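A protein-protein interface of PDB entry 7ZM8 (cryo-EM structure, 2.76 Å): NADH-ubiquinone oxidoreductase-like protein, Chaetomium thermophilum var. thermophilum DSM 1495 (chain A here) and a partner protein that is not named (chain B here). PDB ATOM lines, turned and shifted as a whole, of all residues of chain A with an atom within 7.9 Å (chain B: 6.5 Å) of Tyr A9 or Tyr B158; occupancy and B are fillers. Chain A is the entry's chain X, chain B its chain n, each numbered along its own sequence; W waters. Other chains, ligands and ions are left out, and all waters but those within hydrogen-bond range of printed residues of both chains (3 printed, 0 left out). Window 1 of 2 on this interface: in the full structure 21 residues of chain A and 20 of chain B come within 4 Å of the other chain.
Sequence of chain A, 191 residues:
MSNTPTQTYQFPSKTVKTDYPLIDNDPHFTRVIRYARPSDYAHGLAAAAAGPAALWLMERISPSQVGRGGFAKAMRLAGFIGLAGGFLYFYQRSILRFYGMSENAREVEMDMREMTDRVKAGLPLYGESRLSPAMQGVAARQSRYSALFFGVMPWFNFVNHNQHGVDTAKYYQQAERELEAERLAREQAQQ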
ATOM      1  N   THR A   6      -7.783 -15.853 -22.559  1.00  0.00           N
ATOM      2  CA  THR A   6      -7.596 -15.165 -23.875  1.00  0.00           C
ATOM      3  C   THR A   6      -8.508 -13.936 -23.993  1.00  0.00           C
ATOM      4  O   THR A   6      -8.459 -13.279 -25.050  1.00  0.00           O
ATOM      5  CB  THR A   6      -7.603 -16.109 -25.090  1.00  0.00           C
ATOM      6  OG1 THR A   6      -8.939 -16.461 -25.452  1.00  0.00           O
ATOM      7  CG2 THR A   6      -6.751 -17.346 -24.898  1.00  0.00           C
ATOM      8  N   GLN A   7      -9.300 -13.636 -22.961  1.00  0.00           N
ATOM      9  CA  GLN A   7     -10.128 -12.398 -22.970  1.00  0.00           C
ATOM     10  C   GLN A   7     -10.029 -11.746 -21.590  1.00  0.00           C
ATOM     11  O   GLN A   7     -11.034 -11.764 -20.855  1.00  0.00           O
ATOM     12  CB  GLN A   7     -11.568 -12.715 -23.380  1.00  0.00           C
ATOM     13  CG  GLN A   7     -12.310 -11.516 -23.954  1.00  0.00           C
ATOM     14  CD  GLN A   7     -11.658 -10.964 -25.198  1.00  0.00           C
ATOM     15  OE1 GLN A   7     -11.497  -9.757 -25.353  1.00  0.00           O
ATOM     16  NE2 GLN A   7     -11.272 -11.854 -26.099  1.00  0.00           N
ATOM     17  N   THR A   8      -8.857 -11.212 -21.247  1.00  0.00           N
ATOM     18  CA  THR A   8      -8.643 -10.623 -19.898  1.00  0.00           C
ATOM     19  C   THR A   8      -9.550  -9.401 -19.710  1.00  0.00           C
ATOM     20  O   THR A   8     -10.088  -9.249 -18.601  1.00  0.00           O
ATOM     21  CB  THR A   8      -7.141 -10.493 -19.626  1.00  0.00           C
ATOM     22  OG1 THR A   8      -6.547  -9.824 -20.737  1.00  0.00           O
ATOM     23  CG2 THR A   8      -6.479 -11.842 -19.454  1.00  0.00           C
ATOM     24  N   TYR A   9      -9.696  -8.558 -20.736  1.00  0.00           N
ATOM     25  CA  TYR A   9     -10.663  -7.431 -20.673  1.00  0.00           C
ATOM     26  C   TYR A   9     -11.819  -7.833 -21.588  1.00  0.00           C
ATOM     27  O   TYR A   9     -11.627  -7.821 -22.817  1.00  0.00           O
ATOM     28  CB  TYR A   9      -9.973  -6.153 -21.147  1.00  0.00           C
ATOM     29  CG  TYR A   9     -10.677  -4.850 -20.875  1.00  0.00           C
ATOM     30  CD1 TYR A   9     -11.566  -4.313 -21.792  1.00  0.00           C
ATOM     31  CD2 TYR A   9     -10.413  -4.124 -19.726  1.00  0.00           C
ATOM     32  CE1 TYR A   9     -12.197  -3.102 -21.561  1.00  0.00           C
ATOM     33  CE2 TYR A   9     -11.039  -2.914 -19.477  1.00  0.00           C
ATOM     34  CZ  TYR A   9     -11.934  -2.401 -20.399  1.00  0.00           C
ATOM     35  OH  TYR A   9     -12.552  -1.209 -20.164  1.00  0.00           O
ATOM     36  N   GLN A  10     -12.977  -8.176 -21.022  1.00  0.00           N
ATOM     37  CA  GLN A  10     -14.088  -8.703 -21.856  1.00  0.00           C
ATOM     38  C   GLN A  10     -15.251  -7.711 -21.918  1.00  0.00           C
ATOM     39  O   GLN A  10     -16.115  -7.878 -22.797  1.00  0.00           O
ATOM     40  CB  GLN A  10     -14.554 -10.024 -21.246  1.00  0.00           C
ATOM     41  CG  GLN A  10     -15.487 -10.836 -22.132  1.00  0.00           C
ATOM     42  CD  GLN A  10     -15.931 -12.108 -21.452  1.00  0.00           C
ATOM     43  OE1 GLN A  10     -15.468 -12.448 -20.365  1.00  0.00           O
ATOM     44  NE2 GLN A  10     -16.841 -12.825 -22.093  1.00  0.00           N
ATOM     45  N   PHE A  11     -15.267  -6.707 -21.042  1.00  0.00           N
ATOM     46  CA  PHE A  11     -16.452  -5.812 -20.987  1.00  0.00           C
ATOM     47  C   PHE A  11     -16.031  -4.337 -21.087  1.00  0.00           C
ATOM     48  O   PHE A  11     -15.024  -3.998 -20.452  1.00  0.00           O
ATOM     49  CB  PHE A  11     -17.276  -6.095 -19.727  1.00  0.00           C
ATOM     50  CG  PHE A  11     -17.641  -7.542 -19.515  1.00  0.00           C
ATOM     51  CD1 PHE A  11     -16.876  -8.355 -18.696  1.00  0.00           C
ATOM     52  CD2 PHE A  11     -18.748  -8.093 -20.139  1.00  0.00           C
ATOM     53  CE1 PHE A  11     -17.207  -9.687 -18.508  1.00  0.00           C
ATOM     54  CE2 PHE A  11     -19.079  -9.425 -19.951  1.00  0.00           C
ATOM     55  CZ  PHE A  11     -18.310 -10.219 -19.134  1.00  0.00           C
ATOM     56  N   PRO A  12     -16.751  -3.427 -21.799  1.00  0.00           N
ATOM     57  CA  PRO A  12     -16.338  -2.034 -21.833  1.00  0.00           C
ATOM     58  C   PRO A  12     -16.553  -1.447 -20.432  1.00  0.00           C
ATOM     59  O   PRO A  12     -17.608  -1.616 -19.879  1.00  0.00           O
ATOM     60  CB  PRO A  12     -17.225  -1.430 -22.933  1.00  0.00           C
ATOM     61  CG  PRO A  12     -18.463  -2.296 -22.936  1.00  0.00           C
ATOM     62  CD  PRO A  12     -17.981  -3.678 -22.550  1.00  0.00           C
ATOM     63  N   SER A  13     -15.560  -0.743 -19.899  1.00  0.00           N
ATOM     64  CA  SER A  13     -15.664  -0.244 -18.507  1.00  0.00           C
ATOM     65  C   SER A  13     -15.307   1.231 -18.485  1.00  0.00           C
ATOM     66  O   SER A  13     -14.614   1.664 -19.408  1.00  0.00           O
ATOM     67  CB  SER A  13     -14.781  -1.036 -17.582  1.00  0.00           C
ATOM     68  OG  SER A  13     -15.305  -1.038 -16.266  1.00  0.00           O
ATOM     69  N   LYS A  14     -15.805   1.961 -17.491  1.00  0.00           N
ATOM     70  CA  LYS A  14     -15.482   3.403 -17.360  1.00  0.00           C
ATOM     71  C   LYS A  14     -14.117   3.589 -16.702  1.00  0.00           C
ATOM     72  O   LYS A  14     -13.912   3.012 -15.631  1.00  0.00           O
ATOM     73  CB  LYS A  14     -16.554   4.109 -16.529  1.00  0.00           C
ATOM     74  CG  LYS A  14     -16.333   5.590 -16.261  1.00  0.00           C
ATOM     75  CD  LYS A  14     -16.483   6.455 -17.487  1.00  0.00           C
ATOM     76  CE  LYS A  14     -16.461   7.928 -17.148  1.00  0.00           C
ATOM     77  NZ  LYS A  14     -16.537   8.775 -18.361  1.00  0.00           N
ATOM     78  N   THR A  15     -13.219   4.352 -17.326  1.00  0.00           N
ATOM     79  CA  THR A  15     -11.931   4.694 -16.672  1.00  0.00           C
ATOM     80  C   THR A  15     -12.145   6.007 -15.913  1.00  0.00           C
ATOM     81  O   THR A  15     -12.679   6.958 -16.512  1.00  0.00           O
ATOM     82  CB  THR A  15     -10.773   4.790 -17.679  1.00  0.00           C
ATOM     83  OG1 THR A  15     -10.459   3.475 -18.132  1.00  0.00           O
ATOM     84  CG2 THR A  15      -9.532   5.435 -17.110  1.00  0.00           C
ATOM     85  N   ASN A  25     -13.647  -2.231  -9.662  1.00  0.00           N
ATOM     86  CA  ASN A  25     -14.682  -1.187  -9.874  1.00  0.00           C
ATOM     87  C   ASN A  25     -15.863  -1.574  -8.986  1.00  0.00           C
ATOM     88  O   ASN A  25     -16.670  -0.689  -8.650  1.00  0.00           O
ATOM     89  CB  ASN A  25     -15.206  -1.184 -11.316  1.00  0.00           C
ATOM     90  CG  ASN A  25     -14.435  -0.298 -12.262  1.00  0.00           C
ATOM     91  OD1 ASN A  25     -13.416   0.266 -11.891  1.00  0.00           O
ATOM     92  ND2 ASN A  25     -14.916  -0.168 -13.488  1.00  0.00           N
ATOM     93  N   ASN A 162     -17.731 -11.376 -12.994  1.00  0.00           N
ATOM     94  CA  ASN A 162     -16.332 -11.140 -13.406  1.00  0.00           C
ATOM     95  C   ASN A 162     -16.174  -9.812 -14.147  1.00  0.00           C
ATOM     96  O   ASN A 162     -15.182  -9.674 -14.871  1.00  0.00           O
ATOM     97  CB  ASN A 162     -15.807 -12.318 -14.221  1.00  0.00           C
ATOM     98  CG  ASN A 162     -16.848 -12.943 -15.124  1.00  0.00           C
ATOM     99  OD1 ASN A 162     -17.758 -12.269 -15.599  1.00  0.00           O
ATOM    100  ND2 ASN A 162     -16.712 -14.233 -15.381  1.00  0.00           N
ATOM    101  N   HIS A 164     -15.105  -6.401 -13.317  1.00  0.00           N
ATOM    102  CA  HIS A 164     -14.523  -5.579 -12.213  1.00  0.00           C
ATOM    103  C   HIS A 164     -13.703  -4.402 -12.723  1.00  0.00           C
ATOM    104  O   HIS A 164     -13.028  -3.801 -11.902  1.00  0.00           O
ATOM    105  CB  HIS A 164     -13.781  -6.485 -11.240  1.00  0.00           C
ATOM    106  CG  HIS A 164     -14.702  -7.396 -10.510  1.00  0.00           C
ATOM    107  ND1 HIS A 164     -15.167  -7.110  -9.249  1.00  0.00           N
ATOM    108  CD2 HIS A 164     -15.285  -8.556 -10.873  1.00  0.00           C
ATOM    109  CE1 HIS A 164     -15.974  -8.066  -8.855  1.00  0.00           C
ATOM    110  NE2 HIS A 164     -16.064  -8.961  -9.831  1.00  0.00           N
ATOM    111  N   GLY A 165     -13.721  -4.147 -14.028  1.00  0.00           N
ATOM    112  CA  GLY A 165     -13.052  -2.969 -14.596  1.00  0.00           C
ATOM    113  C   GLY A 165     -11.567  -3.113 -14.824  1.00  0.00           C
ATOM    114  O   GLY A 165     -10.976  -2.143 -15.272  1.00  0.00           O
ATOM    115  N   VAL A 166     -10.991  -4.280 -14.554  1.00  0.00           N
ATOM    116  CA  VAL A 166      -9.517  -4.433 -14.623  1.00  0.00           C
ATOM    117  C   VAL A 166      -9.126  -5.505 -15.637  1.00  0.00           C
ATOM    118  O   VAL A 166      -9.887  -6.464 -15.778  1.00  0.00           O
ATOM    119  CB  VAL A 166      -8.971  -4.753 -13.225  1.00  0.00           C
ATOM    120  CG1 VAL A 166      -8.822  -3.504 -12.374  1.00  0.00           C
ATOM    121  CG2 VAL A 166      -9.810  -5.792 -12.505  1.00  0.00           C
ATOM    122  N   ASP A 167      -8.026  -5.312 -16.368  1.00  0.00           N
ATOM    123  CA  ASP A 167      -7.490  -6.369 -17.276  1.00  0.00           C
ATOM    124  C   ASP A 167      -6.955  -7.444 -16.345  1.00  0.00           C
ATOM    125  O   ASP A 167      -6.310  -7.094 -15.370  1.00  0.00           O
ATOM    126  CB  ASP A 167      -6.381  -5.825 -18.168  1.00  0.00           C
ATOM    127  CG  ASP A 167      -6.351  -6.352 -19.584  1.00  0.00           C
ATOM    128  OD1 ASP A 167      -6.986  -7.375 -19.837  1.00  0.00           O
ATOM    129  OD2 ASP A 167      -5.682  -5.726 -20.421  1.00  0.00           O
ATOM    130  N   THR A 168      -7.235  -8.718 -16.595  1.00  0.00           N
ATOM    131  CA  THR A 168      -6.844  -9.746 -15.592  1.00  0.00           C
ATOM    132  C   THR A 168      -5.556 -10.479 -15.977  1.00  0.00           C
ATOM    133  O   THR A 168      -5.233 -11.466 -15.301  1.00  0.00           O
ATOM    134  CB  THR A 168      -8.032 -10.645 -15.225  1.00  0.00           C
ATOM    135  OG1 THR A 168      -8.523 -11.274 -16.407  1.00  0.00           O
ATOM    136  CG2 THR A 168      -9.150  -9.884 -14.549  1.00  0.00           C
ATOM    137  N   ALA A 169      -4.843  -9.995 -16.991  1.00  0.00           N
ATOM    138  CA  ALA A 169      -3.577 -10.624 -17.420  1.00  0.00           C
ATOM    139  C   ALA A 169      -2.550 -10.625 -16.283  1.00  0.00           C
ATOM    140  O   ALA A 169      -1.942 -11.652 -16.073  1.00  0.00           O
ATOM    141  CB  ALA A 169      -3.056  -9.865 -18.598  1.00  0.00           C
ATOM    142  N   GLU B 128     -17.650  12.028 -23.905  1.00  0.00           N
ATOM    143  CA  GLU B 128     -17.177  10.705 -23.443  1.00  0.00           C
ATOM    144  C   GLU B 128     -18.348  10.115 -22.665  1.00  0.00           C
ATOM    145  O   GLU B 128     -18.933  10.835 -21.849  1.00  0.00           O
ATOM    146  CB  GLU B 128     -15.892  10.816 -22.623  1.00  0.00           C
ATOM    147  CG  GLU B 128     -16.011  11.669 -21.376  1.00  0.00           C
ATOM    148  CD  GLU B 128     -14.687  12.018 -20.719  1.00  0.00           C
ATOM    149  OE1 GLU B 128     -14.710  12.591 -19.611  1.00  0.00           O
ATOM    150  OE2 GLU B 128     -13.636  11.718 -21.317  1.00  0.00           O
ATOM    151  N   LEU B 129     -18.722   8.879 -22.967  1.00  0.00           N
ATOM    152  CA  LEU B 129     -19.912   8.296 -22.323  1.00  0.00           C
ATOM    153  C   LEU B 129     -19.647   8.152 -20.830  1.00  0.00           C
ATOM    154  O   LEU B 129     -18.608   7.586 -20.478  1.00  0.00           O
ATOM    155  CB  LEU B 129     -20.207   6.958 -23.003  1.00  0.00           C
ATOM    156  CG  LEU B 129     -20.705   7.055 -24.440  1.00  0.00           C
ATOM    157  CD1 LEU B 129     -20.691   5.689 -25.099  1.00  0.00           C
ATOM    158  CD2 LEU B 129     -22.102   7.649 -24.473  1.00  0.00           C
ATOM    159  N   TYR B 131     -21.442   6.380 -19.085  1.00  0.00           N
ATOM    160  CA  TYR B 131     -21.841   4.962 -18.902  1.00  0.00           C
ATOM    161  C   TYR B 131     -21.483   4.149 -20.155  1.00  0.00           C
ATOM    162  O   TYR B 131     -22.388   3.811 -20.931  1.00  0.00           O
ATOM    163  CB  TYR B 131     -23.320   4.919 -18.514  1.00  0.00           C
ATOM    164  CG  TYR B 131     -23.904   3.569 -18.192  1.00  0.00           C
ATOM    165  CD1 TYR B 131     -23.496   2.854 -17.080  1.00  0.00           C
ATOM    166  CD2 TYR B 131     -24.906   3.030 -18.980  1.00  0.00           C
ATOM    167  CE1 TYR B 131     -24.049   1.622 -16.776  1.00  0.00           C
ATOM    168  CE2 TYR B 131     -25.467   1.800 -18.694  1.00  0.00           C
ATOM    169  CZ  TYR B 131     -25.036   1.094 -17.588  1.00  0.00           C
ATOM    170  OH  TYR B 131     -25.598  -0.113 -17.300  1.00  0.00           O
ATOM    171  N   PRO B 132     -20.193   3.836 -20.410  1.00  0.00           N
ATOM    172  CA  PRO B 132     -19.777   3.001 -21.554  1.00  0.00           C
ATOM    173  C   PRO B 132     -20.364   1.583 -21.486  1.00  0.00           C
ATOM    174  O   PRO B 132     -20.296   0.898 -22.470  1.00  0.00           O
ATOM    175  CB  PRO B 132     -18.258   2.868 -21.375  1.00  0.00           C
ATOM    176  CG  PRO B 132     -18.010   3.212 -19.938  1.00  0.00           C
ATOM    177  CD  PRO B 132     -19.040   4.271 -19.625  1.00  0.00           C
ATOM    178  N   PHE B 135     -22.891  -0.462 -23.974  1.00  0.00           N
ATOM    179  CA  PHE B 135     -22.514  -1.398 -25.060  1.00  0.00           C
ATOM    180  C   PHE B 135     -22.863  -2.832 -24.656  1.00  0.00           C
ATOM    181  O   PHE B 135     -23.020  -3.685 -25.549  1.00  0.00           O
ATOM    182  CB  PHE B 135     -21.039  -1.221 -25.420  1.00  0.00           C
ATOM    183  CG  PHE B 135     -20.742  -0.002 -26.254  1.00  0.00           C
ATOM    184  CD1 PHE B 135     -21.122   0.053 -27.585  1.00  0.00           C
ATOM    185  CD2 PHE B 135     -20.079   1.086 -25.712  1.00  0.00           C
ATOM    186  CE1 PHE B 135     -20.844   1.171 -28.353  1.00  0.00           C
ATOM    187  CE2 PHE B 135     -19.807   2.206 -26.482  1.00  0.00           C
ATOM    188  CZ  PHE B 135     -20.189   2.245 -27.800  1.00  0.00           C
ATOM    189  N   HIS B 153     -14.011  -3.968 -31.657  1.00  0.00           N
ATOM    190  CA  HIS B 153     -13.211  -2.760 -31.801  1.00  0.00           C
ATOM    191  C   HIS B 153     -13.577  -1.721 -30.755  1.00  0.00           C
ATOM    192  O   HIS B 153     -12.731  -0.912 -30.360  1.00  0.00           O
ATOM    193  CB  HIS B 153     -13.359  -2.189 -33.209  1.00  0.00           C
ATOM    194  CG  HIS B 153     -14.735  -1.695 -33.528  1.00  0.00           C
ATOM    195  ND1 HIS B 153     -14.990  -0.393 -33.895  1.00  0.00           N
ATOM    196  CD2 HIS B 153     -15.930  -2.331 -33.549  1.00  0.00           C
ATOM    197  CE1 HIS B 153     -16.282  -0.245 -34.121  1.00  0.00           C
ATOM    198  NE2 HIS B 153     -16.876  -1.406 -33.916  1.00  0.00           N
ATOM    199  N   VAL B 154     -14.829  -1.720 -30.301  1.00  0.00           N
ATOM    200  CA  VAL B 154     -15.200  -0.910 -29.150  1.00  0.00           C
ATOM    201  C   VAL B 154     -14.486  -1.410 -27.904  1.00  0.00           C
ATOM    202  O   VAL B 154     -13.990  -0.621 -27.096  1.00  0.00           O
ATOM    203  CB  VAL B 154     -16.727  -0.923 -28.969  1.00  0.00           C
ATOM    204  CG1 VAL B 154     -17.145   0.001 -27.848  1.00  0.00           C
ATOM    205  CG2 VAL B 154     -17.404  -0.543 -30.260  1.00  0.00           C
ATOM    206  N   ILE B 155     -14.433  -2.731 -27.731  1.00  0.00           N
ATOM    207  CA  ILE B 155     -13.814  -3.317 -26.548  1.00  0.00           C
ATOM    208  C   ILE B 155     -12.336  -2.974 -26.500  1.00  0.00           C
ATOM    209  O   ILE B 155     -11.795  -2.635 -25.441  1.00  0.00           O
ATOM    210  CB  ILE B 155     -14.037  -4.840 -26.536  1.00  0.00           C
ATOM    211  CG1 ILE B 155     -15.519  -5.167 -26.394  1.00  0.00           C
ATOM    212  CG2 ILE B 155     -13.259  -5.481 -25.407  1.00  0.00           C
ATOM    213  CD1 ILE B 155     -16.003  -5.187 -24.992  1.00  0.00           C
ATOM    214  N   GLU B 156     -11.693  -2.945 -27.661  1.00  0.00           N
ATOM    215  CA  GLU B 156     -10.248  -2.629 -27.718  1.00  0.00           C
ATOM    216  C   GLU B 156      -9.977  -1.152 -27.408  1.00  0.00           C
ATOM    217  O   GLU B 156      -8.941  -0.876 -26.825  1.00  0.00           O
ATOM    218  CB  GLU B 156      -9.675  -3.121 -29.041  1.00  0.00           C
ATOM    219  CG  GLU B 156      -8.184  -3.397 -28.970  1.00  0.00           C
ATOM    220  CD  GLU B 156      -7.746  -4.275 -27.806  1.00  0.00           C
ATOM    221  OE1 GLU B 156      -8.403  -5.307 -27.558  1.00  0.00           O
ATOM    222  OE2 GLU B 156      -6.751  -3.917 -27.144  1.00  0.00           O
ATOM    223  N   HIS B 157     -10.866  -0.242 -27.779  1.00  0.00           N
ATOM    224  CA  HIS B 157     -10.722   1.201 -27.493  1.00  0.00           C
ATOM    225  C   HIS B 157     -10.778   1.423 -25.998  1.00  0.00           C
ATOM    226  O   HIS B 157      -9.995   2.231 -25.487  1.00  0.00           O
ATOM    227  CB  HIS B 157     -11.836   1.967 -28.217  1.00  0.00           C
ATOM    228  CG  HIS B 157     -12.086   3.351 -27.722  1.00  0.00           C
ATOM    229  ND1 HIS B 157     -11.480   4.451 -28.284  1.00  0.00           N
ATOM    230  CD2 HIS B 157     -12.881   3.816 -26.737  1.00  0.00           C
ATOM    231  CE1 HIS B 157     -11.881   5.536 -27.656  1.00  0.00           C
ATOM    232  NE2 HIS B 157     -12.740   5.173 -26.703  1.00  0.00           N
ATOM    233  N   TYR B 158     -11.659   0.696 -25.329  1.00  0.00           N
ATOM    234  CA  TYR B 158     -11.868   0.898 -23.880  1.00  0.00           C
ATOM    235  C   TYR B 158     -10.782   0.120 -23.150  1.00  0.00           C
ATOM    236  O   TYR B 158     -10.447   0.487 -22.038  1.00  0.00           O
ATOM    237  CB  TYR B 158     -13.314   0.512 -23.553  1.00  0.00           C
ATOM    238  CG  TYR B 158     -14.326   1.595 -23.817  1.00  0.00           C
ATOM    239  CD1 TYR B 158     -14.212   2.833 -23.211  1.00  0.00           C
ATOM    240  CD2 TYR B 158     -15.397   1.386 -24.666  1.00  0.00           C
ATOM    241  CE1 TYR B 158     -15.130   3.839 -23.448  1.00  0.00           C
ATOM    242  CE2 TYR B 158     -16.329   2.380 -24.910  1.00  0.00           C
ATOM    243  CZ  TYR B 158     -16.195   3.613 -24.299  1.00  0.00           C
ATOM    244  OH  TYR B 158     -17.104   4.604 -24.526  1.00  0.00           O
ATOM    245  N   ARG B 159     -10.237  -0.919 -23.780  1.00  0.00           N
ATOM    246  CA  ARG B 159      -9.102  -1.589 -23.155  1.00  0.00           C
ATOM    247  C   ARG B 159      -7.854  -0.715 -23.188  1.00  0.00           C
ATOM    248  O   ARG B 159      -7.112  -0.644 -22.204  1.00  0.00           O
ATOM    249  CB  ARG B 159      -8.837  -2.920 -23.846  1.00  0.00           C
ATOM    250  CG  ARG B 159      -7.736  -3.723 -23.207  1.00  0.00           C
ATOM    251  CD  ARG B 159      -7.582  -5.050 -23.884  1.00  0.00           C
ATOM    252  NE  ARG B 159      -6.496  -5.821 -23.298  1.00  0.00           N
ATOM    253  CZ  ARG B 159      -6.148  -7.040 -23.697  1.00  0.00           C
ATOM    254  NH1 ARG B 159      -6.800  -7.624 -24.691  1.00  0.00           N
ATOM    255  NH2 ARG B 159      -5.142  -7.669 -23.107  1.00  0.00           N
ATOM    256  N   LYS B 160      -7.587  -0.093 -24.322  1.00  0.00           N
ATOM    257  CA  LYS B 160      -6.451   0.847 -24.422  1.00  0.00           C
ATOM    258  C   LYS B 160      -6.585   1.890 -23.328  1.00  0.00           C
ATOM    259  O   LYS B 160      -5.583   2.184 -22.701  1.00  0.00           O
ATOM    260  CB  LYS B 160      -6.437   1.543 -25.784  1.00  0.00           C
ATOM    261  CG  LYS B 160      -6.074   0.659 -26.967  1.00  0.00           C
ATOM    262  CD  LYS B 160      -4.837  -0.175 -26.731  1.00  0.00           C
ATOM    263  CE  LYS B 160      -4.480  -1.038 -27.922  1.00  0.00           C
ATOM    264  NZ  LYS B 160      -4.216  -0.218 -29.128  1.00  0.00           N
ATOM    265  N   GLN B 161      -7.759   2.484 -23.172  1.00  0.00           N
ATOM    266  CA  GLN B 161      -7.944   3.605 -22.220  1.00  0.00           C
ATOM    267  C   GLN B 161      -7.637   3.171 -20.792  1.00  0.00           C
ATOM    268  O   GLN B 161      -6.964   3.934 -20.085  1.00  0.00           O
ATOM    269  CB  GLN B 161      -9.354   4.155 -22.404  1.00  0.00           C
ATOM    270  CG  GLN B 161      -9.745   5.248 -21.428  1.00  0.00           C
ATOM    271  CD  GLN B 161     -11.168   5.676 -21.668  1.00  0.00           C
ATOM    272  OE1 GLN B 161     -11.797   5.256 -22.632  1.00  0.00           O
ATOM    273  NE2 GLN B 161     -11.684   6.524 -20.795  1.00  0.00           N
ATOM    274  N   HIS B 162      -8.080   1.984 -20.393  1.00  0.00           N
ATOM    275  CA  HIS B 162      -7.808   1.452 -19.038  1.00  0.00           C
ATOM    276  C   HIS B 162      -6.306   1.257 -18.856  1.00  0.00           C
ATOM    277  O   HIS B 162      -5.800   1.607 -17.787  1.00  0.00           O
ATOM    278  CB  HIS B 162      -8.547   0.119 -18.902  1.00  0.00           C
ATOM    279  CG  HIS B 162      -8.067  -0.737 -17.778  1.00  0.00           C
ATOM    280  ND1 HIS B 162      -8.403  -0.489 -16.465  1.00  0.00           N
ATOM    281  CD2 HIS B 162      -7.279  -1.830 -17.767  1.00  0.00           C
ATOM    282  CE1 HIS B 162      -7.834  -1.382 -15.691  1.00  0.00           C
ATOM    283  NE2 HIS B 162      -7.145  -2.220 -16.467  1.00  0.00           N
ATOM    284  N   LEU B 163      -5.636   0.690 -19.861  1.00  0.00           N
ATOM    285  CA  LEU B 163      -4.188   0.393 -19.803  1.00  0.00           C
ATOM    286  C   LEU B 163      -3.370   1.679 -19.753  1.00  0.00           C
ATOM    287  O   LEU B 163      -2.391   1.719 -19.014  1.00  0.00           O
ATOM    288  CB  LEU B 163      -3.856  -0.488 -21.008  1.00  0.00           C
ATOM    289  CG  LEU B 163      -4.389  -1.919 -20.933  1.00  0.00           C
ATOM    290  CD1 LEU B 163      -4.020  -2.706 -22.179  1.00  0.00           C
ATOM    291  CD2 LEU B 163      -3.887  -2.627 -19.687  1.00  0.00           C
HETATM  292  O   HOH W   1      -9.767   1.871 -15.820  1.00  0.00           O
HETATM  293  O   HOH W   2      -5.633  -4.290 -14.850  1.00  0.00           O
HETATM  294  O   HOH W   3     -12.014   2.262 -20.160  1.00  0.00           O
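Of chain B, only Ile B155, Tyr B158, Arg B159 and His B162 come within 4 Å of Tyr A9. Of the printed residues of chain A, Tyr B158 touches Tyr A9 (3.3 Å), Pro A12 (3.8 Å) and Ser A13 (3.999 Å). Of the printed residues of chain B, Phe A11 touches Ile B155. Of the printed residues of chain A, Leu B163 touches Asp A167 (3.7 Å). Printed residues of chain A within 4 Å of Arg B159: Thr A8 (3.5 Å), Tyr A9 (3.7 Å) and Asp A167 (3.0 Å). Glu B156 touches none of the printed residues of chain A. Lys B160 touches none of the printed residues of chain A. The nearest residue of chain B that does not touch Tyr A9 is Glu B156 (6.0 Å). The nearest printed residue of chain A that does not touch Tyr B158 is Thr A15 (4.9 Å). The nearest printed residue of chain B that does not touch Lys A14 is Glu B128 (4.2 Å).
Printed residues of chain A that touch a printed residue of chain B: Thr A8, Tyr A9, Gln A10, Phe A11, Pro A12, Ser A13, Lys A14, Thr A15, Gly A165, Val A166 and Asp A167. Hydrophobic or aromatic side chains of chain A within 4 Å of the printed part of chain B: Tyr A9 and Pro A12. Of the 16 printed residues of chain B, 9 touch a printed residue of chain A. Hydrophobic or aromatic side chains of chain B that line the printed part of chain A: Pro B132, Phe B135, Ile B155, Tyr B158, His B162 and Leu B163.
Among the printed residues, pairs that only touch across the chains: Thr A15 with His B162 (3.5 Å), Gln A10 with Ile B155 (3.5 Å), Pro A12 with Ile B155 (3.5 Å), Lys A14 with Pro B132 (3.5 Å), Val A166 with His B162 (3.6 Å), Ser A13 with Pro B132 (3.7 Å), Asp A167 with Leu B163 (3.7 Å), Tyr A9 with Arg B159 (3.7 Å), Thr A15 with Gln B161 (3.7 Å), Pro A12 with Pro B132 (3.7 Å), Pro A12 with Phe B135 (3.7 Å), Pro A12 with Tyr B158 (3.8 Å), Tyr A9 with Ile B155 (3.9 Å), Tyr A9 with His B162 (3.97 Å), Phe A11 with Ile B155 (3.997 Å) and Ser A13 with Tyr B158 (3.999 Å).
The side-chain hydroxyl (OG1) of Thr A8 lies within hydrogen-bond range of the guanidinium group (NH2) of Arg B159 (3.5 Å). O of Tyr B158 sits at hydrogen-bond distance from OH of Tyr A9 (3.3 Å). The side-chain amino group of Lys A14 sits at hydrogen-bond distance from the backbone carbonyl oxygen of Leu B129. The backbone carbonyl oxygen (O) of Gly A165 lies close to a ring nitrogen (ND1) of His B162 (3.3 Å). NE of Arg B159 lies within salt-bridge range of OD2 of Asp A167, 3.0 Å away. N of Asp A167 sits at hydrogen-bond distance from NE2 of His B162, at 3.2 Å.
The side-chain amide oxygen (OE1) of Gln A7 lies close to the backbone carbonyl oxygen (O) of Tyr A9, at 3.2 Å. The side-chain hydroxyl (OG1) of Thr A8 lies within hydrogen-bond range of the side-chain carboxylate (OD1) of Asp A167. The side-chain hydroxyl (OG1) of Thr A168 is in hydrogen-bond range of the backbone carbonyl oxygen (O) of Thr A8, at 3.4 Å. OH of Tyr A9 sits at hydrogen-bond distance from N of Ser A13 (3.1 Å). N of Tyr A9 is in hydrogen-bond range of OD1 of Asp A167 (3.1 Å). The side-chain amide nitrogen of Asn A25 lies within hydrogen-bond range of the side-chain hydroxyl of Ser A13 (2.9 Å).
Water W3 lies within hydrogen-bond range of the backbone carbonyl oxygen of Ser A13, the side-chain hydroxyl of Thr A15 and the backbone carbonyl oxygen of Tyr B158. Water W1 bridges a ring nitrogen (ND1) of His B162 (2.8 Å) and the side-chain hydroxyl of Thr A15 (2.9 Å). Water W2 bridges O of Asp A167 and NE2 of His B162.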
